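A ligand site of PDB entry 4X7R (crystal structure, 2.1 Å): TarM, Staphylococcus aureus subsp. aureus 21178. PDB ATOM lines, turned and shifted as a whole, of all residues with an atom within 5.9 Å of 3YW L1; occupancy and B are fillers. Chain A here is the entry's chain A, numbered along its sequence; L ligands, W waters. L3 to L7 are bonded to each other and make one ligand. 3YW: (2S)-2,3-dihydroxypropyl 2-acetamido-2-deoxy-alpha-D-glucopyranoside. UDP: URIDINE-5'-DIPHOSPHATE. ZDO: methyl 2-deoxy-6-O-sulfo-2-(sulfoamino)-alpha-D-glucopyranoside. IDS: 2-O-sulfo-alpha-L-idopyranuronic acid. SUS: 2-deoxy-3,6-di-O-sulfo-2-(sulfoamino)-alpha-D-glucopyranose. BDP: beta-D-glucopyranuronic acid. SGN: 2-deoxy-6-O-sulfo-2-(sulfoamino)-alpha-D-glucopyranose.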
ATOM      1  N   GLY A  16      12.088  14.472  13.846  1.00  0.00           N
ATOM      2  CA  GLY A  16      11.901  15.708  14.594  1.00  0.00           C
ATOM      3  C   GLY A  16      12.556  15.743  15.956  1.00  0.00           C
ATOM      4  O   GLY A  16      13.594  15.113  16.197  1.00  0.00           O
ATOM      5  N   GLY A  17      11.930  16.499  16.852  1.00  0.00           N
ATOM      6  CA  GLY A  17      12.471  16.842  18.164  1.00  0.00           C
ATOM      7  C   GLY A  17      12.682  15.741  19.162  1.00  0.00           C
ATOM      8  O   GLY A  17      13.621  15.843  19.956  1.00  0.00           O
ATOM      9  N   MET A  18      11.827  14.724  19.189  1.00  0.00           N
ATOM     10  CA  MET A  18      11.994  13.669  20.200  1.00  0.00           C
ATOM     11  C   MET A  18      13.292  12.934  20.063  1.00  0.00           C
ATOM     12  O   MET A  18      13.991  12.780  21.056  1.00  0.00           O
ATOM     13  CB  MET A  18      10.786  12.694  20.250  1.00  0.00           C
ATOM     14  CG  MET A  18      11.041  11.419  21.100  1.00  0.00           C
ATOM     15  SD  MET A  18       9.593  10.384  21.381  1.00  0.00           S
ATOM     16  CE  MET A  18       9.304   9.765  19.689  1.00  0.00           C
ATOM     17  N   SER A  21      16.282  15.305  20.706  1.00  0.00           N
ATOM     18  CA  SER A  21      16.579  15.474  22.130  1.00  0.00           C
ATOM     19  C   SER A  21      17.251  14.253  22.739  1.00  0.00           C
ATOM     20  O   SER A  21      18.077  14.404  23.634  1.00  0.00           O
ATOM     21  CB  SER A  21      15.321  15.857  22.913  1.00  0.00           C
ATOM     22  OG  SER A  21      14.492  14.744  23.186  1.00  0.00           O
ATOM     23  N   PRO A 228       6.215   7.459  23.957  1.00  0.00           N
ATOM     24  CA  PRO A 228       5.083   7.168  24.873  1.00  0.00           C
ATOM     25  C   PRO A 228       4.409   5.824  24.683  1.00  0.00           C
ATOM     26  O   PRO A 228       4.036   5.160  25.665  1.00  0.00           O
ATOM     27  CB  PRO A 228       4.125   8.350  24.641  1.00  0.00           C
ATOM     28  CG  PRO A 228       4.482   8.897  23.277  1.00  0.00           C
ATOM     29  CD  PRO A 228       5.970   8.684  23.154  1.00  0.00           C
ATOM     30  N   HIS A 249       7.085  14.211  26.105  1.00  0.00           N
ATOM     31  CA  HIS A 249       7.644  15.190  25.171  1.00  0.00           C
ATOM     32  C   HIS A 249       6.594  16.168  24.626  1.00  0.00           C
ATOM     33  O   HIS A 249       6.948  17.145  23.963  1.00  0.00           O
ATOM     34  CB  HIS A 249       8.344  14.467  24.003  1.00  0.00           C
ATOM     35  CG  HIS A 249       9.624  13.814  24.393  1.00  0.00           C
ATOM     36  ND1 HIS A 249      10.816  14.487  24.307  1.00  0.00           N
ATOM     37  CD2 HIS A 249       9.850  12.558  24.859  1.00  0.00           C
ATOM     38  CE1 HIS A 249      11.742  13.635  24.715  1.00  0.00           C
ATOM     39  NE2 HIS A 249      11.203  12.461  25.060  1.00  0.00           N
ATOM     40  N   VAL A 250       5.334  15.917  24.905  1.00  0.00           N
ATOM     41  CA  VAL A 250       4.238  16.689  24.283  1.00  0.00           C
ATOM     42  C   VAL A 250       3.256  17.257  25.313  1.00  0.00           C
ATOM     43  O   VAL A 250       3.234  16.837  26.469  1.00  0.00           O
ATOM     44  CB  VAL A 250       3.466  15.776  23.264  1.00  0.00           C
ATOM     45  CG1 VAL A 250       4.387  15.224  22.161  1.00  0.00           C
ATOM     46  CG2 VAL A 250       2.775  14.603  23.975  1.00  0.00           C
ATOM     47  N   ASN A 251       2.373  18.122  24.851  1.00  0.00           N
ATOM     48  CA  ASN A 251       1.251  18.575  25.653  1.00  0.00           C
ATOM     49  C   ASN A 251       0.371  17.292  25.801  1.00  0.00           C
ATOM     50  O   ASN A 251       0.049  16.637  24.808  1.00  0.00           O
ATOM     51  CB  ASN A 251       0.504  19.715  24.929  1.00  0.00           C
ATOM     52  CG  ASN A 251      -0.624  20.319  25.731  1.00  0.00           C
ATOM     53  OD1 ASN A 251      -1.302  19.623  26.486  1.00  0.00           O
ATOM     54  ND2 ASN A 251      -0.864  21.620  25.578  1.00  0.00           N
ATOM     55  N   GLU A 266       0.156   9.121  26.969  1.00  0.00           N
ATOM     56  CA  GLU A 266       0.605  10.040  28.011  1.00  0.00           C
ATOM     57  C   GLU A 266      -0.203   9.922  29.282  1.00  0.00           C
ATOM     58  O   GLU A 266       0.373   9.983  30.363  1.00  0.00           O
ATOM     59  CB  GLU A 266       0.650  11.504  27.508  1.00  0.00           C
ATOM     60  CG  GLU A 266       1.806  11.758  26.534  1.00  0.00           C
ATOM     61  CD  GLU A 266       1.661  11.226  25.111  1.00  0.00           C
ATOM     62  OE1 GLU A 266       0.588  10.697  24.771  1.00  0.00           O
ATOM     63  OE2 GLU A 266       2.622  11.374  24.326  1.00  0.00           O
ATOM     64  N   LEU A 282       8.770  18.770  30.343  1.00  0.00           N
ATOM     65  CA  LEU A 282       9.780  19.728  29.947  1.00  0.00           C
ATOM     66  C   LEU A 282       9.658  21.123  30.543  1.00  0.00           C
ATOM     67  O   LEU A 282      10.645  21.853  30.525  1.00  0.00           O
ATOM     68  CB  LEU A 282       9.900  19.783  28.418  1.00  0.00           C
ATOM     69  CG  LEU A 282      10.186  18.425  27.713  1.00  0.00           C
ATOM     70  CD1 LEU A 282       9.816  18.524  26.233  1.00  0.00           C
ATOM     71  CD2 LEU A 282      11.632  17.994  27.911  1.00  0.00           C
ATOM     72  N   ASN A 304      14.721  20.018  28.083  1.00  0.00           N
ATOM     73  CA  ASN A 304      15.594  19.317  27.155  1.00  0.00           C
ATOM     74  C   ASN A 304      16.954  19.997  27.292  1.00  0.00           C
ATOM     75  O   ASN A 304      17.004  21.220  27.544  1.00  0.00           O
ATOM     76  CB  ASN A 304      15.178  19.549  25.707  1.00  0.00           C
ATOM     77  CG  ASN A 304      14.054  18.684  25.242  1.00  0.00           C
ATOM     78  OD1 ASN A 304      14.093  17.478  25.416  1.00  0.00           O
ATOM     79  ND2 ASN A 304      13.021  19.310  24.675  1.00  0.00           N
ATOM     80  N   ARG A 326       8.717  19.248  11.525  1.00  0.00           N
ATOM     81  CA  ARG A 326       8.047  18.085  10.940  1.00  0.00           C
ATOM     82  C   ARG A 326       6.780  18.740  10.359  1.00  0.00           C
ATOM     83  O   ARG A 326       6.186  19.599  11.036  1.00  0.00           O
ATOM     84  CB  ARG A 326       7.615  17.090  12.023  1.00  0.00           C
ATOM     85  CG  ARG A 326       8.715  16.295  12.678  1.00  0.00           C
ATOM     86  CD  ARG A 326       8.150  15.313  13.697  1.00  0.00           C
ATOM     87  NE  ARG A 326       7.506  15.992  14.823  1.00  0.00           N
ATOM     88  CZ  ARG A 326       6.270  15.771  15.232  1.00  0.00           C
ATOM     89  NH1 ARG A 326       5.517  14.864  14.640  1.00  0.00           N
ATOM     90  NH2 ARG A 326       5.767  16.452  16.261  1.00  0.00           N
ATOM     91  N   THR A 330      -0.337  19.623  13.964  1.00  0.00           N
ATOM     92  CA  THR A 330      -0.189  20.455  15.175  1.00  0.00           C
ATOM     93  C   THR A 330       0.637  21.718  14.988  1.00  0.00           C
ATOM     94  O   THR A 330       0.465  22.687  15.731  1.00  0.00           O
ATOM     95  CB  THR A 330       0.244  19.644  16.378  1.00  0.00           C
ATOM     96  OG1 THR A 330       1.511  19.080  16.090  1.00  0.00           O
ATOM     97  CG2 THR A 330      -0.742  18.554  16.748  1.00  0.00           C
ATOM     98  N   LYS A 331       1.506  21.727  13.957  1.00  0.00           N
ATOM     99  CA  LYS A 331       2.380  22.846  13.609  1.00  0.00           C
ATOM    100  C   LYS A 331       1.605  23.964  12.925  1.00  0.00           C
ATOM    101  O   LYS A 331       2.080  25.106  12.866  1.00  0.00           O
ATOM    102  CB  LYS A 331       3.580  22.386  12.755  1.00  0.00           C
ATOM    103  CG  LYS A 331       4.432  21.296  13.410  1.00  0.00           C
ATOM    104  CD  LYS A 331       5.237  21.774  14.624  1.00  0.00           C
ATOM    105  CE  LYS A 331       5.842  20.584  15.323  1.00  0.00           C
ATOM    106  NZ  LYS A 331       6.582  20.987  16.544  1.00  0.00           N
ATOM    107  N   SER A 400       2.463  26.880  15.695  1.00  0.00           N
ATOM    108  CA  SER A 400       2.165  25.624  16.406  1.00  0.00           C
ATOM    109  C   SER A 400       1.144  25.829  17.515  1.00  0.00           C
ATOM    110  O   SER A 400       1.203  26.836  18.225  1.00  0.00           O
ATOM    111  CB  SER A 400       3.438  24.993  16.952  1.00  0.00           C
ATOM    112  OG  SER A 400       3.145  23.701  17.434  1.00  0.00           O
ATOM    113  N   TYR A 402       0.369  23.166  19.762  1.00  0.00           N
ATOM    114  CA  TYR A 402       0.724  22.316  20.893  1.00  0.00           C
ATOM    115  C   TYR A 402       2.215  21.976  20.871  1.00  0.00           C
ATOM    116  O   TYR A 402       2.743  21.571  19.835  1.00  0.00           O
ATOM    117  CB  TYR A 402      -0.109  21.005  20.915  1.00  0.00           C
ATOM    118  CG  TYR A 402      -1.595  21.166  20.632  1.00  0.00           C
ATOM    119  CD1 TYR A 402      -2.500  21.426  21.658  1.00  0.00           C
ATOM    120  CD2 TYR A 402      -2.092  21.060  19.326  1.00  0.00           C
ATOM    121  CE1 TYR A 402      -3.863  21.588  21.397  1.00  0.00           C
ATOM    122  CE2 TYR A 402      -3.450  21.238  19.066  1.00  0.00           C
ATOM    123  CZ  TYR A 402      -4.332  21.489  20.093  1.00  0.00           C
ATOM    124  OH  TYR A 402      -5.658  21.667  19.828  1.00  0.00           O
ATOM    125  N   GLU A 403       2.882  22.108  22.025  1.00  0.00           N
ATOM    126  CA  GLU A 403       4.287  21.733  22.173  1.00  0.00           C
ATOM    127  C   GLU A 403       4.516  21.222  23.596  1.00  0.00           C
ATOM    128  O   GLU A 403       3.760  21.536  24.521  1.00  0.00           O
ATOM    129  CB  GLU A 403       5.246  22.937  21.913  1.00  0.00           C
ATOM    130  CG  GLU A 403       5.287  23.524  20.503  1.00  0.00           C
ATOM    131  CD  GLU A 403       5.794  22.597  19.420  1.00  0.00           C
ATOM    132  OE1 GLU A 403       6.499  21.619  19.738  1.00  0.00           O
ATOM    133  OE2 GLU A 403       5.475  22.860  18.235  1.00  0.00           O
ATOM    134  N   GLY A 404       5.606  20.492  23.737  1.00  0.00           N
ATOM    135  CA  GLY A 404       6.152  20.079  25.014  1.00  0.00           C
ATOM    136  C   GLY A 404       7.124  21.155  25.436  1.00  0.00           C
ATOM    137  O   GLY A 404       7.190  21.537  26.614  1.00  0.00           O
ATOM    138  N   GLN A 405       7.868  21.693  24.458  1.00  0.00           N
ATOM    139  CA  GLN A 405       8.842  22.777  24.682  1.00  0.00           C
ATOM    140  C   GLN A 405       9.119  23.578  23.410  1.00  0.00           C
ATOM    141  O   GLN A 405       8.914  24.781  23.397  1.00  0.00           O
ATOM    142  CB  GLN A 405      10.162  22.236  25.285  1.00  0.00           C
ATOM    143  CG  GLN A 405      11.102  23.347  25.736  1.00  0.00           C
ATOM    144  CD  GLN A 405      12.286  22.839  26.531  1.00  0.00           C
ATOM    145  OE1 GLN A 405      12.829  21.765  26.281  1.00  0.00           O
ATOM    146  NE2 GLN A 405      12.699  23.627  27.515  1.00  0.00           N
ATOM    147  N   GLY A 406       9.659  22.921  22.371  1.00  0.00           N
ATOM    148  CA  GLY A 406       9.930  23.583  21.085  1.00  0.00           C
ATOM    149  C   GLY A 406      11.379  23.860  20.812  1.00  0.00           C
ATOM    150  O   GLY A 406      11.832  25.007  20.894  1.00  0.00           O
ATOM    151  N   LEU A 407      12.118  22.832  20.428  1.00  0.00           N
ATOM    152  CA  LEU A 407      13.534  22.955  20.146  1.00  0.00           C
ATOM    153  C   LEU A 407      13.851  23.859  18.959  1.00  0.00           C
ATOM    154  O   LEU A 407      14.868  24.528  19.018  1.00  0.00           O
ATOM    155  CB  LEU A 407      14.216  21.584  19.997  1.00  0.00           C
ATOM    156  CG  LEU A 407      14.253  20.687  21.255  1.00  0.00           C
ATOM    157  CD1 LEU A 407      14.715  19.268  20.892  1.00  0.00           C
ATOM    158  CD2 LEU A 407      15.195  21.277  22.327  1.00  0.00           C
ATOM    159  N   TYR A 426       2.976  23.934  25.520  1.00  0.00           N
ATOM    160  CA  TYR A 426       3.902  24.538  26.478  1.00  0.00           C
ATOM    161  C   TYR A 426       5.189  24.926  25.796  1.00  0.00           C
ATOM    162  O   TYR A 426       5.574  24.294  24.812  1.00  0.00           O
ATOM    163  CB  TYR A 426       4.239  23.488  27.550  1.00  0.00           C
ATOM    164  CG  TYR A 426       3.032  23.009  28.310  1.00  0.00           C
ATOM    165  CD1 TYR A 426       2.508  23.764  29.362  1.00  0.00           C
ATOM    166  CD2 TYR A 426       2.405  21.804  27.981  1.00  0.00           C
ATOM    167  CE1 TYR A 426       1.384  23.344  30.053  1.00  0.00           C
ATOM    168  CE2 TYR A 426       1.284  21.363  28.693  1.00  0.00           C
ATOM    169  CZ  TYR A 426       0.769  22.136  29.718  1.00  0.00           C
ATOM    170  OH  TYR A 426      -0.330  21.729  30.432  1.00  0.00           O
HETATM  171  O3A 3YW L   1       5.064  12.512  19.595  1.00  0.00           O
HETATM  172  C4A 3YW L   1       8.163  14.602  19.835  1.00  0.00           C
HETATM  173  C5A 3YW L   1       6.779  14.187  19.410  1.00  0.00           C
HETATM  174  O5  3YW L   1       9.575  16.537  21.765  1.00  0.00           O
HETATM  175  C6A 3YW L   1       6.334  12.910  20.082  1.00  0.00           C
HETATM  176  C5  3YW L   1      10.442  17.663  21.630  1.00  0.00           C
HETATM  177  C6  3YW L   1      11.727  17.307  22.346  1.00  0.00           C
HETATM  178  C4  3YW L   1       9.731  18.905  22.175  1.00  0.00           C
HETATM  179  O6  3YW L   1      11.503  17.012  23.715  1.00  0.00           O
HETATM  180  C3  3YW L   1       8.536  19.202  21.277  1.00  0.00           C
HETATM  181  O4  3YW L   1      10.611  20.023  22.161  1.00  0.00           O
HETATM  182  O3  3YW L   1       7.806  20.339  21.732  1.00  0.00           O
HETATM  183  O7  3YW L   1       4.870  18.387  21.196  1.00  0.00           O
HETATM  184  C7  3YW L   1       5.431  18.408  20.104  1.00  0.00           C
HETATM  185  C8  3YW L   1       4.702  18.724  18.846  1.00  0.00           C
HETATM  186  N2  3YW L   1       6.740  18.164  19.983  1.00  0.00           N
HETATM  187  C2  3YW L   1       7.632  17.981  21.115  1.00  0.00           C
HETATM  188  C1  3YW L   1       8.346  16.623  21.047  1.00  0.00           C
HETATM  189  O1  3YW L   1       8.384  16.015  19.787  1.00  0.00           O
HETATM  190  O2  3YW L   1       6.761  14.015  17.990  1.00  0.00           O
HETATM  191  N1  UDP L   2      14.470  19.272  12.153  1.00  0.00           N
HETATM  192  C2  UDP L   2      15.562  19.207  11.296  1.00  0.00           C
HETATM  193  N3  UDP L   2      15.275  19.424   9.969  1.00  0.00           N
HETATM  194  C4  UDP L   2      14.038  19.663   9.414  1.00  0.00           C
HETATM  195  C5  UDP L   2      12.945  19.667  10.353  1.00  0.00           C
HETATM  196  C6  UDP L   2      13.183  19.482  11.665  1.00  0.00           C
HETATM  197  O2  UDP L   2      16.694  18.983  11.683  1.00  0.00           O
HETATM  198  O4  UDP L   2      13.951  19.876   8.192  1.00  0.00           O
HETATM  199  C1' UDP L   2      14.773  19.245  13.604  1.00  0.00           C
HETATM  200  C2' UDP L   2      14.951  20.626  14.232  1.00  0.00           C
HETATM  201  O2' UDP L   2      16.285  21.082  14.081  1.00  0.00           O
HETATM  202  C3' UDP L   2      14.604  20.341  15.694  1.00  0.00           C
HETATM  203  C4' UDP L   2      13.538  19.260  15.591  1.00  0.00           C
HETATM  204  O4' UDP L   2      13.682  18.651  14.281  1.00  0.00           O
HETATM  205  O3' UDP L   2      15.700  19.963  16.539  1.00  0.00           O
HETATM  206  C5' UDP L   2      12.125  19.731  15.795  1.00  0.00           C
HETATM  207  O5' UDP L   2      11.976  19.993  17.209  1.00  0.00           O
HETATM  208  PA  UDP L   2      10.683  20.624  17.910  1.00  0.00           P
HETATM  209  O1A UDP L   2      10.779  20.428  19.367  1.00  0.00           O
HETATM  210  O2A UDP L   2      10.617  22.114  17.556  1.00  0.00           O
HETATM  211  O3A UDP L   2       9.417  19.901  17.343  1.00  0.00           O
HETATM  212  PB  UDP L   2       9.006  18.351  17.210  1.00  0.00           P
HETATM  213  O1B UDP L   2       9.522  17.583  18.398  1.00  0.00           O
HETATM  214  O2B UDP L   2       9.599  17.759  15.922  1.00  0.00           O
HETATM  215  O3B UDP L   2       7.495  18.243  17.189  1.00  0.00           O
HETATM  216  C1  ZDO L   3      -4.741  -4.257  20.079  1.00  0.00           C
HETATM  217  C1M ZDO L   3      -5.246  -6.579  20.337  1.00  0.00           C
HETATM  218  C2  ZDO L   3      -4.557  -3.142  19.021  1.00  0.00           C
HETATM  219  C3  ZDO L   3      -3.116  -3.101  18.531  1.00  0.00           C
HETATM  220  C4  ZDO L   3      -2.068  -3.041  19.670  1.00  0.00           C
HETATM  221  C5  ZDO L   3      -2.383  -4.131  20.749  1.00  0.00           C
HETATM  222  C6  ZDO L   3      -1.500  -3.985  22.009  1.00  0.00           C
HETATM  223  O1  ZDO L   3      -4.698  -5.577  19.474  1.00  0.00           O
HETATM  224  N2  ZDO L   3      -5.458  -3.297  17.887  1.00  0.00           N
HETATM  225  S2  ZDO L   3      -6.942  -2.369  18.072  1.00  0.00           S
HETATM  226  OSA ZDO L   3      -7.560  -2.698  19.437  1.00  0.00           O
HETATM  227  OSB ZDO L   3      -7.842  -2.763  16.891  1.00  0.00           O
HETATM  228  OSC ZDO L   3      -6.627  -0.873  18.005  1.00  0.00           O
HETATM  229  O3  ZDO L   3      -2.991  -2.006  17.625  1.00  0.00           O
HETATM  230  O4  ZDO L   3      -0.791  -3.300  19.057  1.00  0.00           O
HETATM  231  O5  ZDO L   3      -3.785  -4.058  21.162  1.00  0.00           O
HETATM  232  O6  ZDO L   3      -1.937  -4.899  23.032  1.00  0.00           O
HETATM  233  S6  ZDO L   3      -1.440  -6.353  23.151  1.00  0.00           S
HETATM  234  OS1 ZDO L   3      -2.434  -7.140  24.018  1.00  0.00           O
HETATM  235  OS2 ZDO L   3      -0.074  -6.360  23.839  1.00  0.00           O
HETATM  236  OS3 ZDO L   3      -1.334  -7.036  21.772  1.00  0.00           O
HETATM  237  C1  IDS L   4       0.301  -2.440  19.420  1.00  0.00           C
HETATM  238  C2  IDS L   4       1.610  -3.057  18.877  1.00  0.00           C
HETATM  239  C3  IDS L   4       1.833  -2.714  17.354  1.00  0.00           C
HETATM  240  C4  IDS L   4       1.544  -1.244  17.021  1.00  0.00           C
HETATM  241  C5  IDS L   4       0.175  -0.811  17.601  1.00  0.00           C
HETATM  242  C6  IDS L   4      -0.123   0.676  17.333  1.00  0.00           C
HETATM  243  O2  IDS L   4       2.734  -2.626  19.690  1.00  0.00           O
HETATM  244  O3  IDS L   4       1.027  -3.538  16.492  1.00  0.00           O
HETATM  245  O4  IDS L   4       2.559  -0.424  17.590  1.00  0.00           O
HETATM  246  O5  IDS L   4       0.198  -1.039  19.039  1.00  0.00           O
HETATM  247  O6A IDS L   4      -0.206   1.420  18.334  1.00  0.00           O
HETATM  248  O6B IDS L   4      -0.247   1.032  16.136  1.00  0.00           O
HETATM  249  S   IDS L   4       3.252  -3.444  20.883  1.00  0.00           S
HETATM  250  O1S IDS L   4       2.135  -3.957  21.797  1.00  0.00           O
HETATM  251  O2S IDS L   4       4.040  -4.622  20.332  1.00  0.00           O
HETATM  252  O3S IDS L   4       4.159  -2.565  21.739  1.00  0.00           O
HETATM  253  N2  SUS L   5       5.124  -0.595  18.685  1.00  0.00           N
HETATM  254  C1  SUS L   5       3.695  -0.287  16.703  1.00  0.00           C
HETATM  255  S1  SUS L   5       6.517  -1.606  18.328  1.00  0.00           S
HETATM  256  C2  SUS L   5       4.838   0.273  17.530  1.00  0.00           C
HETATM  257  S2  SUS L   5       4.153   3.583  12.726  1.00  0.00           S
HETATM  258  C3  SUS L   5       4.507   1.723  17.974  1.00  0.00           C
HETATM  259  O3  SUS L   5       5.634   2.305  18.667  1.00  0.00           O
HETATM  260  S3  SUS L   5       5.495   2.633  20.149  1.00  0.00           S
HETATM  261  C4  SUS L   5       4.090   2.624  16.806  1.00  0.00           C
HETATM  262  O4  SUS L   5       3.599   3.803  17.404  1.00  0.00           O
HETATM  263  C5  SUS L   5       2.975   1.919  15.952  1.00  0.00           C
HETATM  264  O5  SUS L   5       3.430   0.579  15.570  1.00  0.00           O
HETATM  265  C6  SUS L   5       2.687   2.602  14.618  1.00  0.00           C
HETATM  266  O6  SUS L   5       3.909   2.640  13.887  1.00  0.00           O
HETATM  267  O1S SUS L   5       7.762  -0.721  18.219  1.00  0.00           O
HETATM  268  O2S SUS L   5       6.630  -2.604  19.466  1.00  0.00           O
HETATM  269  O3S SUS L   5       6.321  -2.336  16.998  1.00  0.00           O
HETATM  270  O4S SUS L   5       5.641   3.522  12.369  1.00  0.00           O
HETATM  271  O5S SUS L   5       3.278   3.130  11.552  1.00  0.00           O
HETATM  272  O6S SUS L   5       3.787   5.017  13.132  1.00  0.00           O
HETATM  273  O7S SUS L   5       4.301   3.569  20.288  1.00  0.00           O
HETATM  274  O8S SUS L   5       6.737   3.336  20.684  1.00  0.00           O
HETATM  275  O9S SUS L   5       5.235   1.361  20.953  1.00  0.00           O
HETATM  276  C1  BDP L   6       4.030   4.948  16.655  1.00  0.00           C
HETATM  277  C2  BDP L   6       2.881   5.994  16.667  1.00  0.00           C
HETATM  278  C3  BDP L   6       3.333   7.288  15.982  1.00  0.00           C
HETATM  279  C4  BDP L   6       4.748   7.758  16.503  1.00  0.00           C
HETATM  280  C5  BDP L   6       5.750   6.567  16.454  1.00  0.00           C
HETATM  281  C6  BDP L   6       7.158   6.940  16.977  1.00  0.00           C
HETATM  282  O2  BDP L   6       1.752   5.462  15.983  1.00  0.00           O
HETATM  283  O3  BDP L   6       2.340   8.309  16.202  1.00  0.00           O
HETATM  284  O4  BDP L   6       5.223   8.773  15.608  1.00  0.00           O
HETATM  285  O5  BDP L   6       5.234   5.458  17.242  1.00  0.00           O
HETATM  286  O6A BDP L   6       7.280   7.122  18.213  1.00  0.00           O
HETATM  287  O6B BDP L   6       8.095   6.953  16.142  1.00  0.00           O
HETATM  288  C1  SGN L   7       5.308  10.073  16.241  1.00  0.00           C
HETATM  289  C2  SGN L   7       4.889  11.152  15.202  1.00  0.00           C
HETATM  290  C3  SGN L   7       5.911  11.255  14.022  1.00  0.00           C
HETATM  291  C4  SGN L   7       7.367  11.320  14.520  1.00  0.00           C
HETATM  292  C5  SGN L   7       7.650  10.235  15.593  1.00  0.00           C
HETATM  293  C6  SGN L   7       9.071  10.341  16.140  1.00  0.00           C
HETATM  294  N2  SGN L   7       3.535  10.886  14.708  1.00  0.00           N
HETATM  295  O3  SGN L   7       5.647  12.431  13.230  1.00  0.00           O
HETATM  296  O4  SGN L   7       8.283  11.161  13.420  1.00  0.00           O
HETATM  297  O5  SGN L   7       6.675  10.299  16.692  1.00  0.00           O
HETATM  298  O6  SGN L   7       9.222  11.645  16.707  1.00  0.00           O
HETATM  299  S1  SGN L   7       2.370  11.958  15.408  1.00  0.00           S
HETATM  300  O1S SGN L   7       2.658  13.386  14.954  1.00  0.00           O
HETATM  301  O2S SGN L   7       2.429  11.889  16.948  1.00  0.00           O
HETATM  302  O3S SGN L   7       0.990  11.503  14.926  1.00  0.00           O
HETATM  303  S2  SGN L   7      10.307  12.582  16.201  1.00  0.00           S
HETATM  304  O4S SGN L   7      10.034  13.953  16.829  1.00  0.00           O
HETATM  305  O5S SGN L   7      10.325  12.713  14.683  1.00  0.00           O
HETATM  306  O6S SGN L   7      11.634  12.003  16.689  1.00  0.00           O
HETATM  307  O   HOH W   1       2.359  11.778  21.626  1.00  0.00           O
HETATM  308  O   HOH W   2       3.058  20.878  17.206  1.00  0.00           O
HETATM  309  O   HOH W   3       2.448  19.050  22.111  1.00  0.00           O
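The backbone NH (N) of Gly 404 sits at hydrogen-bond distance from an oxygen (O3) of 3YW L1, at 3.0 Å.
O4 of 3YW L1 lies within hydrogen-bond range of N of Gly 406.
The backbone NH (N) of Gly 17 sits at hydrogen-bond distance from an oxygen (O2B) of UDP L2 (2.8 Å).
NH2 of Arg 326 lies within hydrogen-bond range of O2 of 3YW L1.
The guanidinium group (NH1) of Arg 326 lies within salt-bridge range of an oxygen (O1S) of SGN L7 (3.2 Å).
O3B of UDP L2 lies within salt-bridge range of NH2 of Arg 326.
O3 of 3YW L1 is in hydrogen-bond range of OE1 of Glu 403, 2.7 Å away.
An oxygen (O6) of 3YW L1 is in hydrogen-bond range of the side-chain amide nitrogen (ND2) of Asn 304 (2.9 Å).
The side-chain amino group of Lys 331 is in salt-bridge range of an oxygen (O3B) of UDP L2, at 3.0 Å.
The backbone NH of Gly 16 sits at hydrogen-bond distance from an oxygen (O5S) of SGN L7 (2.6 Å).
The backbone NH (N) of Leu 407 is in hydrogen-bond range of an oxygen (O1A) of UDP L2 (2.9 Å).
O3 of 3YW L1 is in hydrogen-bond range of N of Gln 405, at 3.0 Å.
O4S of SGN L7 sits at hydrogen-bond distance from N of Met 18, at 3.1 Å.
ND1 of His 249 sits at hydrogen-bond distance from O6 of 3YW L1 (2.7 Å).
The backbone NH (N) of Gly 17 sits at hydrogen-bond distance from an oxygen (O4S) of SGN L7, 3.2 Å away.
An oxygen (O4) of 3YW L1 lies within hydrogen-bond range of an oxygen (O1A) of UDP L2, 2.8 Å away.
O2 of 3YW L1 lies within hydrogen-bond range of O4S of SGN L7.
N of Gln 405 is in hydrogen-bond range of O of Tyr 426 (3.5 Å).
OG of Ser 21 sits at hydrogen-bond distance from O of Met 18, at 2.9 Å.
The side-chain hydroxyl (OG) of Ser 400 is in hydrogen-bond range of the backbone carbonyl oxygen (O) of Tyr 402 (3.2 Å).
The side-chain amino group (NZ) of Lys 331 lies within salt-bridge range of the side-chain carboxylate (OE2) of Glu 403 (2.8 Å).
The side-chain carboxylate (OE2) of Glu 403 sits at hydrogen-bond distance from the side-chain hydroxyl (OG) of Ser 400 (2.6 Å).
The backbone carbonyl oxygen (O) of Lys 331 is in hydrogen-bond range of the backbone NH (N) of Ser 400, 3.4 Å away.
The side-chain amide nitrogen (ND2) of Asn 304 lies within hydrogen-bond range of the side-chain amide oxygen (OE1) of Gln 405 (2.9 Å).
The backbone carbonyl oxygen (O) of Glu 403 lies within hydrogen-bond range of the backbone NH (N) of Tyr 426, 2.7 Å away.
Gly 17 touches 3YW L1.
Met 18 touches 3YW L1 (CB to C4A, 3.3 Å).
Ser 21 touches 3YW L1 (OG to O6, 3.8 Å).
Val 250 touches 3YW L1.
CD1 of Leu 282 touches O6 of 3YW L1 (3.4 Å).
Lys 331 touches 3YW L1 (NZ to C8, 3.7 Å).
O of Tyr 402 touches C8 of 3YW L1 (3.6 Å).
Leu 407 touches 3YW L1 (N to O4, 3.6 Å).
Hydrophobic or aromatic side chains that line 3YW L1: Met 18, His 249, Val 250, Leu 282 and Leu 407.
Within 4 Å of 3YW L1: Gly 17, Met 18, Ser 21, His 249, Val 250, Leu 282, Asn 304, Arg 326, Lys 331, Tyr 402, Glu 403, Gly 404, Gln 405, Gly 406 and Leu 407.
Water W3 lies within hydrogen-bond range of O7 of 3YW L1 (2.7 Å), N of Asn 251 (2.9 Å), N of Glu 403 (3.1 Å) and O of Tyr 402 (3.4 Å).
Water W2 lies within hydrogen-bond range of OG1 of Thr 330 (2.6 Å), O of Tyr 402 (2.7 Å), OG of Ser 400 (2.8 Å) and OE2 of Glu 403 (3.3 Å).
Water W1 bridges the side-chain carboxylate of Glu 266 (2.7 Å) and an oxygen (O3A) of 3YW L1 (3.5 Å).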
